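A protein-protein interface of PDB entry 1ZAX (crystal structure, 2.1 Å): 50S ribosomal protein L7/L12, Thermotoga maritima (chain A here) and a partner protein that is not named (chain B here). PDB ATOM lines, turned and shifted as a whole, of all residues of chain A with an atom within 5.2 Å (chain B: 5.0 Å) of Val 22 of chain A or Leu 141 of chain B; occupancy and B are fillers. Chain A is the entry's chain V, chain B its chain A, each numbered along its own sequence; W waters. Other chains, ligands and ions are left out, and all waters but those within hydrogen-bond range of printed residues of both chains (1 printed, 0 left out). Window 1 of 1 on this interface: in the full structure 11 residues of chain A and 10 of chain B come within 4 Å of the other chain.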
ATOM      1  N   VAL A  15     -24.972  31.355 -11.313  1.00  0.00           N
ATOM      2  CA  VAL A  15     -24.242  31.011 -12.529  1.00  0.00           C
ATOM      3  C   VAL A  15     -24.407  29.512 -12.816  1.00  0.00           C
ATOM      4  O   VAL A  15     -24.603  29.098 -13.958  1.00  0.00           O
ATOM      5  CB  VAL A  15     -22.737  31.351 -12.397  1.00  0.00           C
ATOM      6  CG1 VAL A  15     -22.132  30.607 -11.217  1.00  0.00           C
ATOM      7  CG2 VAL A  15     -22.003  30.977 -13.673  1.00  0.00           C
ATOM      8  N   GLU A  17     -26.922  27.461 -11.869  1.00  0.00           N
ATOM      9  CA  GLU A  17     -28.292  27.180 -12.302  1.00  0.00           C
ATOM     10  C   GLU A  17     -28.526  27.664 -13.734  1.00  0.00           C
ATOM     11  O   GLU A  17     -29.205  27.007 -14.527  1.00  0.00           O
ATOM     12  CB  GLU A  17     -29.273  27.855 -11.342  1.00  0.00           C
ATOM     13  CG  GLU A  17     -29.304  27.180  -9.971  1.00  0.00           C
ATOM     14  CD  GLU A  17     -30.012  28.002  -8.902  1.00  0.00           C
ATOM     15  OE1 GLU A  17     -30.269  27.442  -7.817  1.00  0.00           O
ATOM     16  OE2 GLU A  17     -30.297  29.195  -9.134  1.00  0.00           O
ATOM     17  N   LEU A  18     -27.946  28.814 -14.054  1.00  0.00           N
ATOM     18  CA  LEU A  18     -28.062  29.396 -15.383  1.00  0.00           C
ATOM     19  C   LEU A  18     -27.458  28.439 -16.419  1.00  0.00           C
ATOM     20  O   LEU A  18     -28.004  28.263 -17.513  1.00  0.00           O
ATOM     21  CB  LEU A  18     -27.336  30.744 -15.414  1.00  0.00           C
ATOM     22  CG  LEU A  18     -27.613  31.687 -16.577  1.00  0.00           C
ATOM     23  CD1 LEU A  18     -29.120  31.934 -16.683  1.00  0.00           C
ATOM     24  CD2 LEU A  18     -26.863  32.999 -16.348  1.00  0.00           C
ATOM     25  N   ALA A  19     -26.342  27.810 -16.058  1.00  0.00           N
ATOM     26  CA  ALA A  19     -25.671  26.871 -16.948  1.00  0.00           C
ATOM     27  C   ALA A  19     -26.556  25.647 -17.206  1.00  0.00           C
ATOM     28  O   ALA A  19     -26.590  25.115 -18.321  1.00  0.00           O
ATOM     29  CB  ALA A  19     -24.329  26.442 -16.346  1.00  0.00           C
ATOM     30  N   GLU A  20     -27.269  25.215 -16.169  1.00  0.00           N
ATOM     31  CA  GLU A  20     -28.175  24.073 -16.263  1.00  0.00           C
ATOM     32  C   GLU A  20     -29.371  24.405 -17.166  1.00  0.00           C
ATOM     33  O   GLU A  20     -29.787  23.586 -17.982  1.00  0.00           O
ATOM     34  CB  GLU A  20     -28.683  23.680 -14.871  1.00  0.00           C
ATOM     35  CG  GLU A  20     -29.586  22.453 -14.876  1.00  0.00           C
ATOM     36  CD  GLU A  20     -30.110  22.103 -13.498  1.00  0.00           C
ATOM     37  OE1 GLU A  20     -29.288  21.945 -12.568  1.00  0.00           O
ATOM     38  OE2 GLU A  20     -31.344  21.979 -13.346  1.00  0.00           O
ATOM     39  N   LEU A  21     -29.918  25.605 -16.998  1.00  0.00           N
ATOM     40  CA  LEU A  21     -31.048  26.070 -17.792  1.00  0.00           C
ATOM     41  C   LEU A  21     -30.637  26.156 -19.263  1.00  0.00           C
ATOM     42  O   LEU A  21     -31.375  25.732 -20.149  1.00  0.00           O
ATOM     43  CB  LEU A  21     -31.509  27.446 -17.303  1.00  0.00           C
ATOM     44  CG  LEU A  21     -32.509  28.203 -18.190  1.00  0.00           C
ATOM     45  CD1 LEU A  21     -33.721  27.323 -18.472  1.00  0.00           C
ATOM     46  CD2 LEU A  21     -32.920  29.511 -17.516  1.00  0.00           C
ATOM     47  N   VAL A  22     -29.448  26.700 -19.515  1.00  0.00           N
ATOM     48  CA  VAL A  22     -28.951  26.820 -20.882  1.00  0.00           C
ATOM     49  C   VAL A  22     -28.765  25.435 -21.512  1.00  0.00           C
ATOM     50  O   VAL A  22     -29.158  25.215 -22.652  1.00  0.00           O
ATOM     51  CB  VAL A  22     -27.609  27.592 -20.919  1.00  0.00           C
ATOM     52  CG1 VAL A  22     -26.920  27.385 -22.255  1.00  0.00           C
ATOM     53  CG2 VAL A  22     -27.860  29.078 -20.685  1.00  0.00           C
ATOM     54  N   LYS A  23     -28.182  24.505 -20.759  1.00  0.00           N
ATOM     55  CA  LYS A  23     -27.946  23.161 -21.271  1.00  0.00           C
ATOM     56  C   LYS A  23     -29.247  22.401 -21.530  1.00  0.00           C
ATOM     57  O   LYS A  23     -29.379  21.703 -22.543  1.00  0.00           O
ATOM     58  CB  LYS A  23     -27.063  22.370 -20.305  1.00  0.00           C
ATOM     59  CG  LYS A  23     -26.832  20.923 -20.743  1.00  0.00           C
ATOM     60  CD  LYS A  23     -26.393  20.854 -22.210  1.00  0.00           C
ATOM     61  CE  LYS A  23     -26.186  19.415 -22.676  1.00  0.00           C
ATOM     62  NZ  LYS A  23     -25.005  18.762 -22.034  1.00  0.00           N
ATOM     63  N   LYS A  24     -30.204  22.536 -20.619  1.00  0.00           N
ATOM     64  CA  LYS A  24     -31.487  21.871 -20.777  1.00  0.00           C
ATOM     65  C   LYS A  24     -32.281  22.420 -21.963  1.00  0.00           C
ATOM     66  O   LYS A  24     -32.891  21.657 -22.713  1.00  0.00           O
ATOM     67  CB  LYS A  24     -32.303  21.977 -19.490  1.00  0.00           C
ATOM     68  CG  LYS A  24     -31.841  21.011 -18.422  1.00  0.00           C
ATOM     69  CD  LYS A  24     -32.758  21.015 -17.210  1.00  0.00           C
ATOM     70  CE  LYS A  24     -32.255  20.032 -16.163  1.00  0.00           C
ATOM     71  NZ  LYS A  24     -33.153  19.939 -14.988  1.00  0.00           N
ATOM     72  N   LEU A  25     -32.260  23.739 -22.137  1.00  0.00           N
ATOM     73  CA  LEU A  25     -32.969  24.388 -23.245  1.00  0.00           C
ATOM     74  C   LEU A  25     -32.356  23.906 -24.559  1.00  0.00           C
ATOM     75  O   LEU A  25     -33.034  23.737 -25.574  1.00  0.00           O
ATOM     76  CB  LEU A  25     -32.815  25.907 -23.134  1.00  0.00           C
ATOM     77  CG  LEU A  25     -34.032  26.818 -22.956  1.00  0.00           C
ATOM     78  CD1 LEU A  25     -35.195  26.084 -22.327  1.00  0.00           C
ATOM     79  CD2 LEU A  25     -33.612  28.001 -22.117  1.00  0.00           C
ATOM     80  N   GLU A  26     -31.050  23.687 -24.512  1.00  0.00           N
ATOM     81  CA  GLU A  26     -30.285  23.226 -25.658  1.00  0.00           C
ATOM     82  C   GLU A  26     -30.802  21.866 -26.129  1.00  0.00           C
ATOM     83  O   GLU A  26     -31.085  21.675 -27.308  1.00  0.00           O
ATOM     84  CB  GLU A  26     -28.816  23.135 -25.252  1.00  0.00           C
ATOM     85  CG  GLU A  26     -27.845  22.876 -26.361  1.00  0.00           C
ATOM     86  CD  GLU A  26     -26.417  22.916 -25.852  1.00  0.00           C
ATOM     87  OE1 GLU A  26     -26.038  23.941 -25.248  1.00  0.00           O
ATOM     88  OE2 GLU A  26     -25.680  21.926 -26.047  1.00  0.00           O
ATOM     89  N   PRO B 136     -18.779  29.197 -19.328  1.00  0.00           N
ATOM     90  CA  PRO B 136     -18.570  30.500 -19.968  1.00  0.00           C
ATOM     91  C   PRO B 136     -18.826  31.535 -18.859  1.00  0.00           C
ATOM     92  O   PRO B 136     -19.374  31.189 -17.805  1.00  0.00           O
ATOM     93  CB  PRO B 136     -19.629  30.529 -21.077  1.00  0.00           C
ATOM     94  CG  PRO B 136     -20.713  29.654 -20.557  1.00  0.00           C
ATOM     95  CD  PRO B 136     -19.992  28.529 -19.842  1.00  0.00           C
ATOM     96  N   SER B 137     -18.403  32.779 -19.064  1.00  0.00           N
ATOM     97  CA  SER B 137     -18.632  33.819 -18.056  1.00  0.00           C
ATOM     98  C   SER B 137     -20.142  33.929 -17.874  1.00  0.00           C
ATOM     99  O   SER B 137     -20.909  33.412 -18.695  1.00  0.00           O
ATOM    100  CB  SER B 137     -18.109  35.174 -18.536  1.00  0.00           C
ATOM    101  OG  SER B 137     -18.884  35.621 -19.637  1.00  0.00           O
ATOM    102  N   LYS B 138     -20.570  34.605 -16.811  1.00  0.00           N
ATOM    103  CA  LYS B 138     -22.002  34.768 -16.566  1.00  0.00           C
ATOM    104  C   LYS B 138     -22.607  35.631 -17.666  1.00  0.00           C
ATOM    105  O   LYS B 138     -23.743  35.412 -18.093  1.00  0.00           O
ATOM    106  CB  LYS B 138     -22.257  35.407 -15.197  1.00  0.00           C
ATOM    107  CG  LYS B 138     -23.725  35.329 -14.751  1.00  0.00           C
ATOM    108  CD  LYS B 138     -23.884  35.660 -13.270  1.00  0.00           C
ATOM    109  CE  LYS B 138     -25.256  35.233 -12.736  1.00  0.00           C
ATOM    110  NZ  LYS B 138     -25.356  35.459 -11.262  1.00  0.00           N
ATOM    111  N   GLU B 139     -21.844  36.610 -18.131  1.00  0.00           N
ATOM    112  CA  GLU B 139     -22.328  37.466 -19.199  1.00  0.00           C
ATOM    113  C   GLU B 139     -22.557  36.628 -20.458  1.00  0.00           C
ATOM    114  O   GLU B 139     -23.568  36.786 -21.139  1.00  0.00           O
ATOM    115  CB  GLU B 139     -21.327  38.590 -19.489  1.00  0.00           C
ATOM    116  CG  GLU B 139     -21.686  39.424 -20.717  1.00  0.00           C
ATOM    117  CD  GLU B 139     -20.874  40.710 -20.833  1.00  0.00           C
ATOM    118  OE1 GLU B 139     -21.136  41.651 -20.050  1.00  0.00           O
ATOM    119  OE2 GLU B 139     -19.977  40.781 -21.703  1.00  0.00           O
ATOM    120  N   GLU B 140     -21.623  35.735 -20.766  1.00  0.00           N
ATOM    121  CA  GLU B 140     -21.784  34.897 -21.950  1.00  0.00           C
ATOM    122  C   GLU B 140     -22.946  33.932 -21.757  1.00  0.00           C
ATOM    123  O   GLU B 140     -23.644  33.610 -22.712  1.00  0.00           O
ATOM    124  CB  GLU B 140     -20.498  34.110 -22.278  1.00  0.00           C
ATOM    125  CG  GLU B 140     -20.622  33.302 -23.587  1.00  0.00           C
ATOM    126  CD  GLU B 140     -19.303  32.737 -24.112  1.00  0.00           C
ATOM    127  OE1 GLU B 140     -19.358  31.846 -24.990  1.00  0.00           O
ATOM    128  OE2 GLU B 140     -18.219  33.176 -23.666  1.00  0.00           O
ATOM    129  N   LEU B 141     -23.158  33.476 -20.523  1.00  0.00           N
ATOM    130  CA  LEU B 141     -24.263  32.554 -20.250  1.00  0.00           C
ATOM    131  C   LEU B 141     -25.597  33.214 -20.584  1.00  0.00           C
ATOM    132  O   LEU B 141     -26.510  32.561 -21.098  1.00  0.00           O
ATOM    133  CB  LEU B 141     -24.248  32.094 -18.782  1.00  0.00           C
ATOM    134  CG  LEU B 141     -23.376  30.860 -18.521  1.00  0.00           C
ATOM    135  CD1 LEU B 141     -23.208  30.641 -17.037  1.00  0.00           C
ATOM    136  CD2 LEU B 141     -24.015  29.624 -19.179  1.00  0.00           C
ATOM    137  N   TYR B 142     -25.700  34.510 -20.297  1.00  0.00           N
ATOM    138  CA  TYR B 142     -26.914  35.270 -20.581  1.00  0.00           C
ATOM    139  C   TYR B 142     -27.110  35.400 -22.090  1.00  0.00           C
ATOM    140  O   TYR B 142     -28.238  35.307 -22.590  1.00  0.00           O
ATOM    141  CB  TYR B 142     -26.833  36.657 -19.937  1.00  0.00           C
ATOM    142  CG  TYR B 142     -27.172  36.666 -18.463  1.00  0.00           C
ATOM    143  CD1 TYR B 142     -26.483  37.491 -17.570  1.00  0.00           C
ATOM    144  CD2 TYR B 142     -28.191  35.859 -17.962  1.00  0.00           C
ATOM    145  CE1 TYR B 142     -26.804  37.508 -16.203  1.00  0.00           C
ATOM    146  CE2 TYR B 142     -28.523  35.868 -16.612  1.00  0.00           C
ATOM    147  CZ  TYR B 142     -27.824  36.694 -15.736  1.00  0.00           C
ATOM    148  OH  TYR B 142     -28.155  36.684 -14.404  1.00  0.00           O
ATOM    149  N   ALA B 143     -26.017  35.630 -22.815  1.00  0.00           N
ATOM    150  CA  ALA B 143     -26.105  35.730 -24.273  1.00  0.00           C
ATOM    151  C   ALA B 143     -26.583  34.367 -24.796  1.00  0.00           C
ATOM    152  O   ALA B 143     -27.489  34.288 -25.615  1.00  0.00           O
ATOM    153  CB  ALA B 143     -24.734  36.078 -24.874  1.00  0.00           C
ATOM    154  N   MET B 144     -25.972  33.299 -24.299  1.00  0.00           N
ATOM    155  CA  MET B 144     -26.334  31.950 -24.709  1.00  0.00           C
ATOM    156  C   MET B 144     -27.803  31.634 -24.428  1.00  0.00           C
ATOM    157  O   MET B 144     -28.478  31.032 -25.263  1.00  0.00           O
ATOM    158  CB  MET B 144     -25.433  30.935 -24.007  1.00  0.00           C
ATOM    159  CG  MET B 144     -23.989  30.972 -24.506  1.00  0.00           C
ATOM    160  SD  MET B 144     -22.890  29.994 -23.471  1.00  0.00           S
ATOM    161  CE  MET B 144     -23.157  28.334 -24.124  1.00  0.00           C
ATOM    162  N   LEU B 145     -28.279  32.035 -23.251  1.00  0.00           N
ATOM    163  CA  LEU B 145     -29.670  31.815 -22.860  1.00  0.00           C
ATOM    164  C   LEU B 145     -30.607  32.468 -23.879  1.00  0.00           C
ATOM    165  O   LEU B 145     -31.574  31.853 -24.324  1.00  0.00           O
ATOM    166  CB  LEU B 145     -29.935  32.405 -21.468  1.00  0.00           C
ATOM    167  CG  LEU B 145     -31.401  32.491 -21.002  1.00  0.00           C
ATOM    168  CD1 LEU B 145     -32.081  31.127 -21.124  1.00  0.00           C
ATOM    169  CD2 LEU B 145     -31.439  32.976 -19.558  1.00  0.00           C
ATOM    170  N   ARG B 148     -30.709  30.378 -26.950  1.00  0.00           N
ATOM    171  CA  ARG B 148     -31.423  29.122 -26.727  1.00  0.00           C
ATOM    172  C   ARG B 148     -32.931  29.340 -26.746  1.00  0.00           C
ATOM    173  O   ARG B 148     -33.676  28.555 -27.324  1.00  0.00           O
ATOM    174  CB  ARG B 148     -31.037  28.517 -25.378  1.00  0.00           C
ATOM    175  CG  ARG B 148     -29.948  27.474 -25.438  1.00  0.00           C
ATOM    176  CD  ARG B 148     -28.684  28.012 -26.070  1.00  0.00           C
ATOM    177  NE  ARG B 148     -27.559  27.121 -25.813  1.00  0.00           N
ATOM    178  CZ  ARG B 148     -26.318  27.315 -26.248  1.00  0.00           C
ATOM    179  NH1 ARG B 148     -25.378  26.429 -25.946  1.00  0.00           N
ATOM    180  NH2 ARG B 148     -26.015  28.379 -26.985  1.00  0.00           N
HETATM  181  O   HOH W   1     -32.619  26.085 -27.325  1.00  0.00           O
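Water W1 lies within hydrogen-bond range of the backbone carbonyl oxygen of Arg 148 of chain B (2.7 Å) and the backbone carbonyl oxygen of Leu 25 of chain A (3.0 Å).
The guanidinium group (NH1) of Arg 148 of chain B lies within salt-bridge range of the side-chain carboxylate (OE1) of Glu 26 of chain A.
Val 22 of chain A touches just these residues of chain B: Leu 141, Leu 145 and Arg 148.
Of the printed residues of chain A, Leu 141 of chain B touches Val 15, Leu 18, Ala 19 and Val 22.
Printed residues of chain B within 4 Å of Leu 18 of chain A: Leu 141, Tyr 142 and Leu 145.
Of the printed residues of chain B, Leu 25 of chain A touches Leu 145 and Arg 148.
Printed residues of chain B within 4 Å of Glu 26 of chain A: Arg 148 (2.7 Å).
Of the printed residues of chain A, Tyr 142 of chain B touches Leu 18.
Pro 136 of chain B touches none of the printed residues of chain A.
Glu 17 of chain A touches none of the printed residues of chain B.
The nearest printed residue of chain A that does not touch Leu 141 of chain B is Glu 20 of chain A (6.3 Å).
Of the 11 printed residues of chain B, 4 touch a printed residue of chain A.
Hydrophobic or aromatic side chains of chain B within 4 Å of the printed part of chain A: Leu 141, Tyr 142 and Leu 145.
Among the printed residues, 11 pairs touch across the chains.
Among the printed residues, Asp or Glu carboxylates within 4 Å of a Lys or Arg side-chain nitrogen of the other chain: Glu 26 of chain A with Arg 148 of chain B.
Val 15 of chain A touches Leu 141 of chain B (CG2 to CD1, 3.6 Å).
CB of Leu 141 of chain B touches CD2 of Leu 18 of chain A, 3.7 Å away.
Leu 18 of chain A touches Tyr 142 of chain B.
Leu 18 of chain A touches Leu 145 of chain B (CD1 to CD2, 3.8 Å).
Leu 141 of chain B touches Ala 19 of chain A.
Val 22 of chain A touches Leu 141 of chain B (CG2 to O, 3.8 Å).
CA of Leu 145 of chain B touches CG2 of Val 22 of chain A, 3.9 Å away.
Val 22 of chain A touches Arg 148 of chain B.
Leu 25 of chain A touches Leu 145 of chain B.
Arg 148 of chain B touches Leu 25 of chain A.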
